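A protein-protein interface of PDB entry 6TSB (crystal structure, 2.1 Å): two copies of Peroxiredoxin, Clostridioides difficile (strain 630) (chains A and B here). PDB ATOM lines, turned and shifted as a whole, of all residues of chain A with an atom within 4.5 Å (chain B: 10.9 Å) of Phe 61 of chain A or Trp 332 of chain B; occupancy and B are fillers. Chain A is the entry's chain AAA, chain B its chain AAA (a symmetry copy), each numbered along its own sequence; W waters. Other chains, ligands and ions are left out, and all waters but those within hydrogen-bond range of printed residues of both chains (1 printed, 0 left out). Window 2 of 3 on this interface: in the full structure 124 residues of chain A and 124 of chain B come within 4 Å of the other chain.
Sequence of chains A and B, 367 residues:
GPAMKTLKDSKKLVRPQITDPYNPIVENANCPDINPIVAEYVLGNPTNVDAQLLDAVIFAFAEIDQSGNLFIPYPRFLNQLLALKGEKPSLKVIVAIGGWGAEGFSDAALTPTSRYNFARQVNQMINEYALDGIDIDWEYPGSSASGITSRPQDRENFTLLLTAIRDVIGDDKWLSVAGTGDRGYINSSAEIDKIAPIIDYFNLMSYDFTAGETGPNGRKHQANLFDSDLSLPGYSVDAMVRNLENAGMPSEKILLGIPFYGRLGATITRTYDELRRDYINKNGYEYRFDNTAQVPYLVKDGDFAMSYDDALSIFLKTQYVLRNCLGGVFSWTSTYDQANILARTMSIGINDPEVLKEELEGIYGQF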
ATOM      1  N   TYR A  41       2.453 -15.610  20.178  1.00  0.00           N
ATOM      2  CA  TYR A  41       1.108 -16.219  20.128  1.00  0.00           C
ATOM      3  C   TYR A  41       1.192 -17.460  21.020  1.00  0.00           C
ATOM      4  O   TYR A  41       2.151 -18.248  20.911  1.00  0.00           O
ATOM      5  CB  TYR A  41       0.643 -16.505  18.682  1.00  0.00           C
ATOM      6  CG  TYR A  41       0.218 -15.272  17.910  1.00  0.00           C
ATOM      7  CD1 TYR A  41       1.150 -14.424  17.323  1.00  0.00           C
ATOM      8  CD2 TYR A  41      -1.113 -14.897  17.811  1.00  0.00           C
ATOM      9  CE1 TYR A  41       0.773 -13.267  16.652  1.00  0.00           C
ATOM     10  CE2 TYR A  41      -1.506 -13.753  17.130  1.00  0.00           C
ATOM     11  CZ  TYR A  41      -0.565 -12.935  16.533  1.00  0.00           C
ATOM     12  OH  TYR A  41      -0.938 -11.795  15.883  1.00  0.00           O
ATOM     13  N   LEU A  43      -1.154 -20.544  21.695  1.00  0.00           N
ATOM     14  CA  LEU A  43      -2.305 -21.415  21.315  1.00  0.00           C
ATOM     15  C   LEU A  43      -2.345 -22.668  22.200  1.00  0.00           C
ATOM     16  O   LEU A  43      -1.526 -23.590  21.982  1.00  0.00           O
ATOM     17  CB  LEU A  43      -2.153 -21.822  19.848  1.00  0.00           C
ATOM     18  CG  LEU A  43      -3.271 -22.698  19.300  1.00  0.00           C
ATOM     19  CD1 LEU A  43      -4.616 -21.976  19.396  1.00  0.00           C
ATOM     20  CD2 LEU A  43      -2.963 -23.159  17.871  1.00  0.00           C
ATOM     21  N   PHE A  59      -2.816 -14.227  23.372  1.00  0.00           N
ATOM     22  CA  PHE A  59      -3.710 -15.397  23.552  1.00  0.00           C
ATOM     23  C   PHE A  59      -4.441 -15.677  22.238  1.00  0.00           C
ATOM     24  O   PHE A  59      -5.126 -14.780  21.716  1.00  0.00           O
ATOM     25  CB  PHE A  59      -4.732 -15.157  24.664  1.00  0.00           C
ATOM     26  CG  PHE A  59      -5.697 -16.308  24.803  1.00  0.00           C
ATOM     27  CD1 PHE A  59      -5.294 -17.505  25.384  1.00  0.00           C
ATOM     28  CD2 PHE A  59      -6.991 -16.217  24.328  1.00  0.00           C
ATOM     29  CE1 PHE A  59      -6.167 -18.576  25.498  1.00  0.00           C
ATOM     30  CE2 PHE A  59      -7.862 -17.295  24.433  1.00  0.00           C
ATOM     31  CZ  PHE A  59      -7.446 -18.475  25.007  1.00  0.00           C
ATOM     32  N   ALA A  60      -4.377 -16.910  21.757  1.00  0.00           N
ATOM     33  CA  ALA A  60      -5.140 -17.367  20.579  1.00  0.00           C
ATOM     34  C   ALA A  60      -6.069 -18.539  20.946  1.00  0.00           C
ATOM     35  O   ALA A  60      -5.614 -19.549  21.478  1.00  0.00           O
ATOM     36  CB  ALA A  60      -4.140 -17.734  19.519  1.00  0.00           C
ATOM     37  N   PHE A  61      -7.376 -18.435  20.666  1.00  0.00           N
ATOM     38  CA  PHE A  61      -8.042 -17.275  20.080  1.00  0.00           C
ATOM     39  C   PHE A  61      -9.384 -16.993  20.778  1.00  0.00           C
ATOM     40  O   PHE A  61      -9.900 -17.861  21.429  1.00  0.00           O
ATOM     41  CB  PHE A  61      -8.427 -17.532  18.620  1.00  0.00           C
ATOM     42  CG  PHE A  61      -7.296 -17.741  17.659  1.00  0.00           C
ATOM     43  CD1 PHE A  61      -6.588 -16.663  17.168  1.00  0.00           C
ATOM     44  CD2 PHE A  61      -6.983 -19.008  17.194  1.00  0.00           C
ATOM     45  CE1 PHE A  61      -5.559 -16.857  16.257  1.00  0.00           C
ATOM     46  CE2 PHE A  61      -5.960 -19.199  16.277  1.00  0.00           C
ATOM     47  CZ  PHE A  61      -5.248 -18.119  15.809  1.00  0.00           C
ATOM     48  N   ALA A  62      -9.932 -15.786  20.654  1.00  0.00           N
ATOM     49  CA  ALA A  62     -11.386 -15.544  20.792  1.00  0.00           C
ATOM     50  C   ALA A  62     -12.019 -15.860  19.429  1.00  0.00           C
ATOM     51  O   ALA A  62     -11.283 -15.791  18.429  1.00  0.00           O
ATOM     52  CB  ALA A  62     -11.649 -14.136  21.250  1.00  0.00           C
ATOM     53  N   GLU A  63     -13.302 -16.232  19.386  1.00  0.00           N
ATOM     54  CA  GLU A  63     -14.033 -16.513  18.125  1.00  0.00           C
ATOM     55  C   GLU A  63     -15.331 -15.685  18.059  1.00  0.00           C
ATOM     56  O   GLU A  63     -15.657 -14.984  19.053  1.00  0.00           O
ATOM     57  CB  GLU A  63     -14.251 -18.025  17.967  1.00  0.00           C
ATOM     58  CG  GLU A  63     -12.975 -18.854  17.807  1.00  0.00           C
ATOM     59  CD  GLU A  63     -11.965 -18.448  16.723  1.00  0.00           C
ATOM     60  OE1 GLU A  63     -12.271 -17.549  15.892  1.00  0.00           O
ATOM     61  OE2 GLU A  63     -10.841 -19.033  16.701  1.00  0.00           O
ATOM     62  N   ILE A  72     -14.664 -16.860  24.152  1.00  0.00           N
ATOM     63  CA  ILE A  72     -13.377 -17.580  24.370  1.00  0.00           C
ATOM     64  C   ILE A  72     -13.683 -19.074  24.476  1.00  0.00           C
ATOM     65  O   ILE A  72     -14.241 -19.513  25.462  1.00  0.00           O
ATOM     66  CB  ILE A  72     -12.704 -17.129  25.686  1.00  0.00           C
ATOM     67  CG1 ILE A  72     -12.921 -15.653  26.056  1.00  0.00           C
ATOM     68  CG2 ILE A  72     -11.239 -17.521  25.671  1.00  0.00           C
ATOM     69  CD1 ILE A  72     -11.954 -14.656  25.452  1.00  0.00           C
ATOM     70  N   PRO A  73     -13.323 -19.941  23.516  1.00  0.00           N
ATOM     71  CA  PRO A  73     -13.503 -21.379  23.708  1.00  0.00           C
ATOM     72  C   PRO A  73     -12.874 -21.977  24.988  1.00  0.00           C
ATOM     73  O   PRO A  73     -13.444 -22.909  25.503  1.00  0.00           O
ATOM     74  CB  PRO A  73     -12.848 -22.021  22.472  1.00  0.00           C
ATOM     75  CG  PRO A  73     -12.700 -20.910  21.446  1.00  0.00           C
ATOM     76  CD  PRO A  73     -12.799 -19.596  22.187  1.00  0.00           C
ATOM     77  N   ALA A  96      -6.118 -12.376  20.537  1.00  0.00           N
ATOM     78  CA  ALA A  96      -6.303 -12.492  19.093  1.00  0.00           C
ATOM     79  C   ALA A  96      -7.694 -13.068  18.845  1.00  0.00           C
ATOM     80  O   ALA A  96      -8.051 -14.099  19.473  1.00  0.00           O
ATOM     81  CB  ALA A  96      -5.228 -13.357  18.501  1.00  0.00           C
ATOM     82  N   GLY A  98      -9.877 -14.626  15.866  1.00  0.00           N
ATOM     83  CA  GLY A  98      -9.987 -15.146  14.497  1.00  0.00           C
ATOM     84  C   GLY A  98      -9.040 -16.297  14.262  1.00  0.00           C
ATOM     85  O   GLY A  98      -9.100 -17.268  15.041  1.00  0.00           O
ATOM     86  N   GLY A  99      -8.238 -16.209  13.194  1.00  0.00           N
ATOM     87  CA  GLY A  99      -7.332 -17.287  12.774  1.00  0.00           C
ATOM     88  C   GLY A  99      -7.833 -17.992  11.544  1.00  0.00           C
ATOM     89  O   GLY A  99      -8.964 -17.725  11.091  1.00  0.00           O
ATOM     90  N   ASP A 137      -7.342 -11.151  13.642  1.00  0.00           N
ATOM     91  CA  ASP A 137      -6.781 -12.177  12.729  1.00  0.00           C
ATOM     92  C   ASP A 137      -7.843 -12.587  11.717  1.00  0.00           C
ATOM     93  O   ASP A 137      -8.198 -13.761  11.652  1.00  0.00           O
ATOM     94  CB  ASP A 137      -6.232 -13.422  13.418  1.00  0.00           C
ATOM     95  CG  ASP A 137      -5.013 -13.170  14.285  1.00  0.00           C
ATOM     96  OD1 ASP A 137      -4.946 -12.076  14.872  1.00  0.00           O
ATOM     97  OD2 ASP A 137      -4.147 -14.097  14.381  1.00  0.00           O
ATOM     98  N   TYR A 207       5.468 -16.551   7.054  1.00  0.00           N
ATOM     99  CA  TYR A 207       5.633 -18.028   7.086  1.00  0.00           C
ATOM    100  C   TYR A 207       4.477 -18.662   6.327  1.00  0.00           C
ATOM    101  O   TYR A 207       3.693 -17.927   5.726  1.00  0.00           O
ATOM    102  CB  TYR A 207       5.754 -18.564   8.514  1.00  0.00           C
ATOM    103  CG  TYR A 207       4.761 -18.019   9.506  1.00  0.00           C
ATOM    104  CD1 TYR A 207       3.463 -18.510   9.578  1.00  0.00           C
ATOM    105  CD2 TYR A 207       5.127 -17.009  10.388  1.00  0.00           C
ATOM    106  CE1 TYR A 207       2.556 -18.012  10.503  1.00  0.00           C
ATOM    107  CE2 TYR A 207       4.224 -16.494  11.299  1.00  0.00           C
ATOM    108  CZ  TYR A 207       2.936 -16.989  11.350  1.00  0.00           C
ATOM    109  OH  TYR A 207       2.063 -16.445  12.236  1.00  0.00           O
ATOM    110  N   ILE A 258       8.051 -15.378  13.085  1.00  0.00           N
ATOM    111  CA  ILE A 258       8.885 -16.601  12.897  1.00  0.00           C
ATOM    112  C   ILE A 258       8.049 -17.821  13.269  1.00  0.00           C
ATOM    113  O   ILE A 258       7.482 -17.871  14.361  1.00  0.00           O
ATOM    114  CB  ILE A 258      10.146 -16.499  13.765  1.00  0.00           C
ATOM    115  CG1 ILE A 258      10.863 -15.168  13.514  1.00  0.00           C
ATOM    116  CG2 ILE A 258      11.063 -17.705  13.556  1.00  0.00           C
ATOM    117  CD1 ILE A 258      11.926 -14.857  14.522  1.00  0.00           C
ATOM    118  N   PRO A 259       8.018 -18.867  12.417  1.00  0.00           N
ATOM    119  CA  PRO A 259       7.363 -20.131  12.751  1.00  0.00           C
ATOM    120  C   PRO A 259       8.236 -20.985  13.682  1.00  0.00           C
ATOM    121  O   PRO A 259       9.425 -21.080  13.401  1.00  0.00           O
ATOM    122  CB  PRO A 259       7.246 -20.839  11.396  1.00  0.00           C
ATOM    123  CG  PRO A 259       8.469 -20.372  10.647  1.00  0.00           C
ATOM    124  CD  PRO A 259       8.677 -18.933  11.108  1.00  0.00           C
ATOM    125  N   PHE A 260       7.646 -21.547  14.750  1.00  0.00           N
ATOM    126  CA  PHE A 260       8.295 -22.497  15.686  1.00  0.00           C
ATOM    127  C   PHE A 260       7.806 -23.886  15.321  1.00  0.00           C
ATOM    128  O   PHE A 260       7.697 -24.750  16.174  1.00  0.00           O
ATOM    129  CB  PHE A 260       7.990 -22.139  17.134  1.00  0.00           C
ATOM    130  CG  PHE A 260       8.789 -20.988  17.678  1.00  0.00           C
ATOM    131  CD1 PHE A 260       9.632 -20.240  16.877  1.00  0.00           C
ATOM    132  CD2 PHE A 260       8.672 -20.625  19.003  1.00  0.00           C
ATOM    133  CE1 PHE A 260      10.358 -19.179  17.415  1.00  0.00           C
ATOM    134  CE2 PHE A 260       9.398 -19.573  19.543  1.00  0.00           C
ATOM    135  CZ  PHE A 260      10.247 -18.854  18.744  1.00  0.00           C
ATOM    136  N   TYR A 261       7.483 -24.061  14.055  1.00  0.00           N
ATOM    137  CA  TYR A 261       7.136 -25.369  13.464  1.00  0.00           C
ATOM    138  C   TYR A 261       7.883 -25.474  12.142  1.00  0.00           C
ATOM    139  O   TYR A 261       8.390 -24.440  11.687  1.00  0.00           O
ATOM    140  CB  TYR A 261       5.634 -25.504  13.201  1.00  0.00           C
ATOM    141  CG  TYR A 261       5.036 -24.457  12.291  1.00  0.00           C
ATOM    142  CD1 TYR A 261       4.692 -23.209  12.777  1.00  0.00           C
ATOM    143  CD2 TYR A 261       4.780 -24.728  10.957  1.00  0.00           C
ATOM    144  CE1 TYR A 261       4.145 -22.239  11.953  1.00  0.00           C
ATOM    145  CE2 TYR A 261       4.208 -23.783  10.123  1.00  0.00           C
ATOM    146  CZ  TYR A 261       3.904 -22.528  10.626  1.00  0.00           C
ATOM    147  OH  TYR A 261       3.355 -21.565   9.837  1.00  0.00           O
ATOM    148  N   SER B 307      11.074 -27.608   6.009  1.00  0.00           N
ATOM    149  CA  SER B 307      11.423 -26.168   6.136  1.00  0.00           C
ATOM    150  C   SER B 307      11.067 -25.672   7.547  1.00  0.00           C
ATOM    151  O   SER B 307       9.900 -25.766   7.941  1.00  0.00           O
ATOM    152  CB  SER B 307      10.708 -25.347   5.083  1.00  0.00           C
ATOM    153  OG  SER B 307      11.047 -23.961   5.169  1.00  0.00           O
ATOM    154  N   TYR B 308      12.022 -25.120   8.272  1.00  0.00           N
ATOM    155  CA  TYR B 308      11.795 -24.582   9.633  1.00  0.00           C
ATOM    156  C   TYR B 308      12.775 -23.434   9.849  1.00  0.00           C
ATOM    157  O   TYR B 308      13.438 -23.059   8.871  1.00  0.00           O
ATOM    158  CB  TYR B 308      11.893 -25.702  10.673  1.00  0.00           C
ATOM    159  CG  TYR B 308      13.245 -26.345  10.851  1.00  0.00           C
ATOM    160  CD1 TYR B 308      13.765 -27.197   9.888  1.00  0.00           C
ATOM    161  CD2 TYR B 308      13.991 -26.140  12.002  1.00  0.00           C
ATOM    162  CE1 TYR B 308      15.011 -27.794  10.039  1.00  0.00           C
ATOM    163  CE2 TYR B 308      15.227 -26.744  12.183  1.00  0.00           C
ATOM    164  CZ  TYR B 308      15.742 -27.573  11.195  1.00  0.00           C
ATOM    165  OH  TYR B 308      16.963 -28.162  11.346  1.00  0.00           O
ATOM    166  N   ASP B 309      12.791 -22.882  11.062  1.00  0.00           N
ATOM    167  CA  ASP B 309      13.772 -21.896  11.579  1.00  0.00           C
ATOM    168  C   ASP B 309      14.527 -22.501  12.789  1.00  0.00           C
ATOM    169  O   ASP B 309      13.890 -23.084  13.726  1.00  0.00           O
ATOM    170  CB  ASP B 309      13.066 -20.578  11.924  1.00  0.00           C
ATOM    171  CG  ASP B 309      12.694 -19.739  10.705  1.00  0.00           C
ATOM    172  OD1 ASP B 309      11.829 -20.184   9.896  1.00  0.00           O
ATOM    173  OD2 ASP B 309      13.301 -18.659  10.546  1.00  0.00           O
ATOM    174  N   ILE B 314      17.076 -17.597  13.020  1.00  0.00           N
ATOM    175  CA  ILE B 314      16.436 -16.638  13.987  1.00  0.00           C
ATOM    176  C   ILE B 314      17.386 -15.488  14.317  1.00  0.00           C
ATOM    177  O   ILE B 314      16.904 -14.330  14.524  1.00  0.00           O
ATOM    178  CB  ILE B 314      15.985 -17.322  15.290  1.00  0.00           C
ATOM    179  CG1 ILE B 314      14.854 -18.321  15.032  1.00  0.00           C
ATOM    180  CG2 ILE B 314      15.607 -16.297  16.355  1.00  0.00           C
ATOM    181  CD1 ILE B 314      14.585 -19.236  16.189  1.00  0.00           C
ATOM    182  N   LYS B 317      17.133 -13.363  11.048  1.00  0.00           N
ATOM    183  CA  LYS B 317      15.818 -12.653  11.090  1.00  0.00           C
ATOM    184  C   LYS B 317      15.860 -11.524  12.126  1.00  0.00           C
ATOM    185  O   LYS B 317      15.422 -10.426  11.760  1.00  0.00           O
ATOM    186  CB  LYS B 317      14.671 -13.642  11.309  1.00  0.00           C
ATOM    187  CG  LYS B 317      14.155 -14.196   9.991  1.00  0.00           C
ATOM    188  CD  LYS B 317      13.408 -15.518  10.057  1.00  0.00           C
ATOM    189  CE  LYS B 317      13.292 -16.104   8.667  1.00  0.00           C
ATOM    190  NZ  LYS B 317      12.235 -17.125   8.582  1.00  0.00           N
ATOM    191  N   VAL B 329       9.694  -8.663  16.932  1.00  0.00           N
ATOM    192  CA  VAL B 329       9.542 -10.024  16.372  1.00  0.00           C
ATOM    193  C   VAL B 329       8.506 -10.748  17.239  1.00  0.00           C
ATOM    194  O   VAL B 329       8.224 -10.292  18.354  1.00  0.00           O
ATOM    195  CB  VAL B 329      10.928 -10.693  16.390  1.00  0.00           C
ATOM    196  CG1 VAL B 329      11.420 -10.928  17.802  1.00  0.00           C
ATOM    197  CG2 VAL B 329      10.966 -11.985  15.602  1.00  0.00           C
ATOM    198  N   PHE B 330       7.959 -11.834  16.728  1.00  0.00           N
ATOM    199  CA  PHE B 330       6.921 -12.650  17.382  1.00  0.00           C
ATOM    200  C   PHE B 330       7.063 -14.038  16.797  1.00  0.00           C
ATOM    201  O   PHE B 330       7.568 -14.138  15.678  1.00  0.00           O
ATOM    202  CB  PHE B 330       5.508 -12.079  17.164  1.00  0.00           C
ATOM    203  CG  PHE B 330       4.833 -12.340  15.830  1.00  0.00           C
ATOM    204  CD1 PHE B 330       4.221 -13.555  15.563  1.00  0.00           C
ATOM    205  CD2 PHE B 330       4.792 -11.354  14.835  1.00  0.00           C
ATOM    206  CE1 PHE B 330       3.562 -13.787  14.364  1.00  0.00           C
ATOM    207  CE2 PHE B 330       4.147 -11.581  13.627  1.00  0.00           C
ATOM    208  CZ  PHE B 330       3.538 -12.801  13.386  1.00  0.00           C
ATOM    209  N   SER B 331       6.607 -15.049  17.531  1.00  0.00           N
ATOM    210  CA  SER B 331       6.565 -16.472  17.104  1.00  0.00           C
ATOM    211  C   SER B 331       5.123 -16.949  17.151  1.00  0.00           C
ATOM    212  O   SER B 331       4.326 -16.406  17.930  1.00  0.00           O
ATOM    213  CB  SER B 331       7.405 -17.379  17.974  1.00  0.00           C
ATOM    214  OG  SER B 331       7.036 -17.264  19.341  1.00  0.00           O
ATOM    215  N   TRP B 332       4.844 -17.875  16.248  1.00  0.00           N
ATOM    216  CA  TRP B 332       3.696 -18.799  16.213  1.00  0.00           C
ATOM    217  C   TRP B 332       4.284 -20.195  16.379  1.00  0.00           C
ATOM    218  O   TRP B 332       4.904 -20.677  15.435  1.00  0.00           O
ATOM    219  CB  TRP B 332       2.940 -18.678  14.879  1.00  0.00           C
ATOM    220  CG  TRP B 332       1.783 -19.617  14.850  1.00  0.00           C
ATOM    221  CD1 TRP B 332       1.760 -20.920  14.443  1.00  0.00           C
ATOM    222  CD2 TRP B 332       0.485 -19.343  15.388  1.00  0.00           C
ATOM    223  NE1 TRP B 332       0.516 -21.456  14.638  1.00  0.00           N
ATOM    224  CE2 TRP B 332      -0.285 -20.510  15.216  1.00  0.00           C
ATOM    225  CE3 TRP B 332      -0.097 -18.215  15.967  1.00  0.00           C
ATOM    226  CZ2 TRP B 332      -1.615 -20.580  15.618  1.00  0.00           C
ATOM    227  CZ3 TRP B 332      -1.411 -18.289  16.368  1.00  0.00           C
ATOM    228  CH2 TRP B 332      -2.152 -19.455  16.191  1.00  0.00           C
ATOM    229  N   THR B 333       4.151 -20.845  17.547  1.00  0.00           N
ATOM    230  CA  THR B 333       3.566 -20.350  18.784  1.00  0.00           C
ATOM    231  C   THR B 333       4.352 -20.990  19.951  1.00  0.00           C
ATOM    232  O   THR B 333       4.917 -22.056  19.723  1.00  0.00           O
ATOM    233  CB  THR B 333       2.075 -20.722  18.804  1.00  0.00           C
ATOM    234  OG1 THR B 333       1.578 -20.424  20.111  1.00  0.00           O
ATOM    235  CG2 THR B 333       1.813 -22.169  18.424  1.00  0.00           C
ATOM    236  N   SER B 334       4.410 -20.383  21.141  1.00  0.00           N
ATOM    237  CA  SER B 334       5.104 -20.922  22.352  1.00  0.00           C
ATOM    238  C   SER B 334       4.832 -22.422  22.580  1.00  0.00           C
ATOM    239  O   SER B 334       5.759 -23.135  22.985  1.00  0.00           O
ATOM    240  CB  SER B 334       4.708 -20.149  23.555  1.00  0.00           C
ATOM    241  OG  SER B 334       3.308 -20.251  23.689  1.00  0.00           O
ATOM    242  N   THR B 335       3.616 -22.881  22.304  1.00  0.00           N
ATOM    243  CA  THR B 335       3.119 -24.274  22.503  1.00  0.00           C
ATOM    244  C   THR B 335       3.896 -25.291  21.669  1.00  0.00           C
ATOM    245  O   THR B 335       3.786 -26.497  21.960  1.00  0.00           O
ATOM    246  CB  THR B 335       1.636 -24.343  22.133  1.00  0.00           C
ATOM    247  OG1 THR B 335       1.048 -23.707  23.263  1.00  0.00           O
ATOM    248  CG2 THR B 335       1.077 -25.736  21.911  1.00  0.00           C
ATOM    249  N   TYR B 336       4.616 -24.852  20.639  1.00  0.00           N
ATOM    250  CA  TYR B 336       5.377 -25.740  19.720  1.00  0.00           C
ATOM    251  C   TYR B 336       6.834 -25.905  20.188  1.00  0.00           C
ATOM    252  O   TYR B 336       7.565 -26.727  19.614  1.00  0.00           O
ATOM    253  CB  TYR B 336       5.316 -25.165  18.308  1.00  0.00           C
ATOM    254  CG  TYR B 336       3.957 -25.154  17.656  1.00  0.00           C
ATOM    255  CD1 TYR B 336       2.845 -25.769  18.221  1.00  0.00           C
ATOM    256  CD2 TYR B 336       3.811 -24.567  16.413  1.00  0.00           C
ATOM    257  CE1 TYR B 336       1.621 -25.781  17.565  1.00  0.00           C
ATOM    258  CE2 TYR B 336       2.592 -24.548  15.760  1.00  0.00           C
ATOM    259  CZ  TYR B 336       1.492 -25.157  16.333  1.00  0.00           C
ATOM    260  OH  TYR B 336       0.317 -25.127  15.637  1.00  0.00           O
ATOM    261  N   ASP B 337       7.210 -25.152  21.219  1.00  0.00           N
ATOM    262  CA  ASP B 337       8.589 -24.905  21.699  1.00  0.00           C
ATOM    263  C   ASP B 337       8.502 -24.892  23.234  1.00  0.00           C
ATOM    264  O   ASP B 337       8.776 -23.828  23.869  1.00  0.00           O
ATOM    265  CB  ASP B 337       9.125 -23.612  21.053  1.00  0.00           C
ATOM    266  CG  ASP B 337      10.460 -23.098  21.587  1.00  0.00           C
ATOM    267  OD1 ASP B 337      11.457 -23.845  21.510  1.00  0.00           O
ATOM    268  OD2 ASP B 337      10.487 -21.951  22.096  1.00  0.00           O
ATOM    269  N   GLN B 338       8.093 -26.035  23.809  1.00  0.00           N
ATOM    270  CA  GLN B 338       7.723 -26.176  25.248  1.00  0.00           C
ATOM    271  C   GLN B 338       8.957 -25.909  26.119  1.00  0.00           C
ATOM    272  O   GLN B 338       8.777 -25.409  27.225  1.00  0.00           O
ATOM    273  CB  GLN B 338       7.095 -27.549  25.522  1.00  0.00           C
ATOM    274  CG  GLN B 338       5.720 -27.774  24.882  1.00  0.00           C
ATOM    275  CD  GLN B 338       4.563 -27.001  25.494  1.00  0.00           C
ATOM    276  OE1 GLN B 338       4.713 -26.224  26.438  1.00  0.00           O
ATOM    277  NE2 GLN B 338       3.373 -27.201  24.943  1.00  0.00           N
ATOM    278  N   LEU B 342      13.745 -22.022  21.013  1.00  0.00           N
ATOM    279  CA  LEU B 342      13.582 -20.987  19.960  1.00  0.00           C
ATOM    280  C   LEU B 342      13.270 -19.636  20.607  1.00  0.00           C
ATOM    281  O   LEU B 342      13.897 -18.668  20.224  1.00  0.00           O
ATOM    282  CB  LEU B 342      12.516 -21.427  18.958  1.00  0.00           C
ATOM    283  CG  LEU B 342      12.841 -22.722  18.230  1.00  0.00           C
ATOM    284  CD1 LEU B 342      11.986 -22.896  16.987  1.00  0.00           C
ATOM    285  CD2 LEU B 342      14.327 -22.809  17.898  1.00  0.00           C
ATOM    286  N   ALA B 343      12.393 -19.600  21.601  1.00  0.00           N
ATOM    287  CA  ALA B 343      11.977 -18.369  22.295  1.00  0.00           C
ATOM    288  C   ALA B 343      13.219 -17.627  22.799  1.00  0.00           C
ATOM    289  O   ALA B 343      13.292 -16.393  22.624  1.00  0.00           O
ATOM    290  CB  ALA B 343      11.023 -18.711  23.414  1.00  0.00           C
ATOM    291  N   MET B 346      15.247 -16.132  19.938  1.00  0.00           N
ATOM    292  CA  MET B 346      14.468 -14.969  19.449  1.00  0.00           C
ATOM    293  C   MET B 346      14.590 -13.806  20.453  1.00  0.00           C
ATOM    294  O   MET B 346      14.835 -12.660  20.023  1.00  0.00           O
ATOM    295  CB  MET B 346      13.009 -15.379  19.223  1.00  0.00           C
ATOM    296  CG  MET B 346      12.165 -14.271  18.682  1.00  0.00           C
ATOM    297  SD  MET B 346      10.507 -14.831  18.267  1.00  0.00           S
ATOM    298  CE  MET B 346       9.810 -14.772  19.917  1.00  0.00           C
HETATM  299  O   HOH W   1      11.314 -23.458  13.458  1.00  0.00           O
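N of Leu 43 of chain A lies within hydrogen-bond range of OG1 of Thr 333 of chain B, 3.2 Å away.
The backbone carbonyl oxygen (O) of Leu 43 of chain A is in hydrogen-bond range of the side-chain hydroxyl (OG1) of Thr 335 of chain B (2.9 Å).
N of Ser 334 of chain B lies within hydrogen-bond range of O of Tyr 41 of chain A, 3.1 Å away.
The backbone NH of Phe 260 of chain A sits at hydrogen-bond distance from the backbone carbonyl oxygen of Trp 332 of chain B (3.0 Å).
O of Ile 258 of chain A is in hydrogen-bond range of N of Trp 332 of chain B (3.2 Å).
O of Tyr 41 of chain A lies close to OG1 of Thr 333 of chain B, 2.4 Å away.
The backbone NH (N) of Ile 258 of chain A is in hydrogen-bond range of the backbone carbonyl oxygen (O) of Phe 330 of chain B, at 2.9 Å.
N of Tyr 41 of chain A is in hydrogen-bond range of O of Ser 331 of chain B, at 3.0 Å.
The side-chain carboxylate of Asp 309 of chain B lies within salt-bridge range of the side-chain amino group of Lys 317 of chain B (2.7 Å).
N of Leu 342 of chain B sits at hydrogen-bond distance from OD1 of Asp 337 of chain B (3.0 Å).
Phe 61 of chain A touches one residue of chain B.
No residue of chain B comes within 4 Å of Ala 62 of chain A.
No residue of chain B comes within 4 Å of Gly 98 of chain A.
No residue of chain B comes within 4 Å of Asp 137 of chain A.
Printed residues of chain B within 4 Å of Phe 260 of chain A: Ser 331, Trp 332, Tyr 336, Asp 337, Leu 342 and Ala 343.
Of the printed residues of chain A, Ser 334 of chain B touches Tyr 41 (3.1 Å).
The nearest residue of chain B that does not touch Phe 61 of chain A is Thr 333 of chain B (8.3 Å).
Of the 18 printed residues of chain A, 8 touch a printed residue of chain B.
Hydrophobic or aromatic side chains of chain B within 4 Å of the printed part of chain A: Tyr 308, Val 329, Phe 330, Trp 332, Tyr 336 and Leu 342.
No position is printed for both chains.
Water W1 lies within hydrogen-bond range of the backbone carbonyl oxygen (O) of Asp 309 of chain B and the backbone carbonyl oxygen (O) of Pro 259 of chain A.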
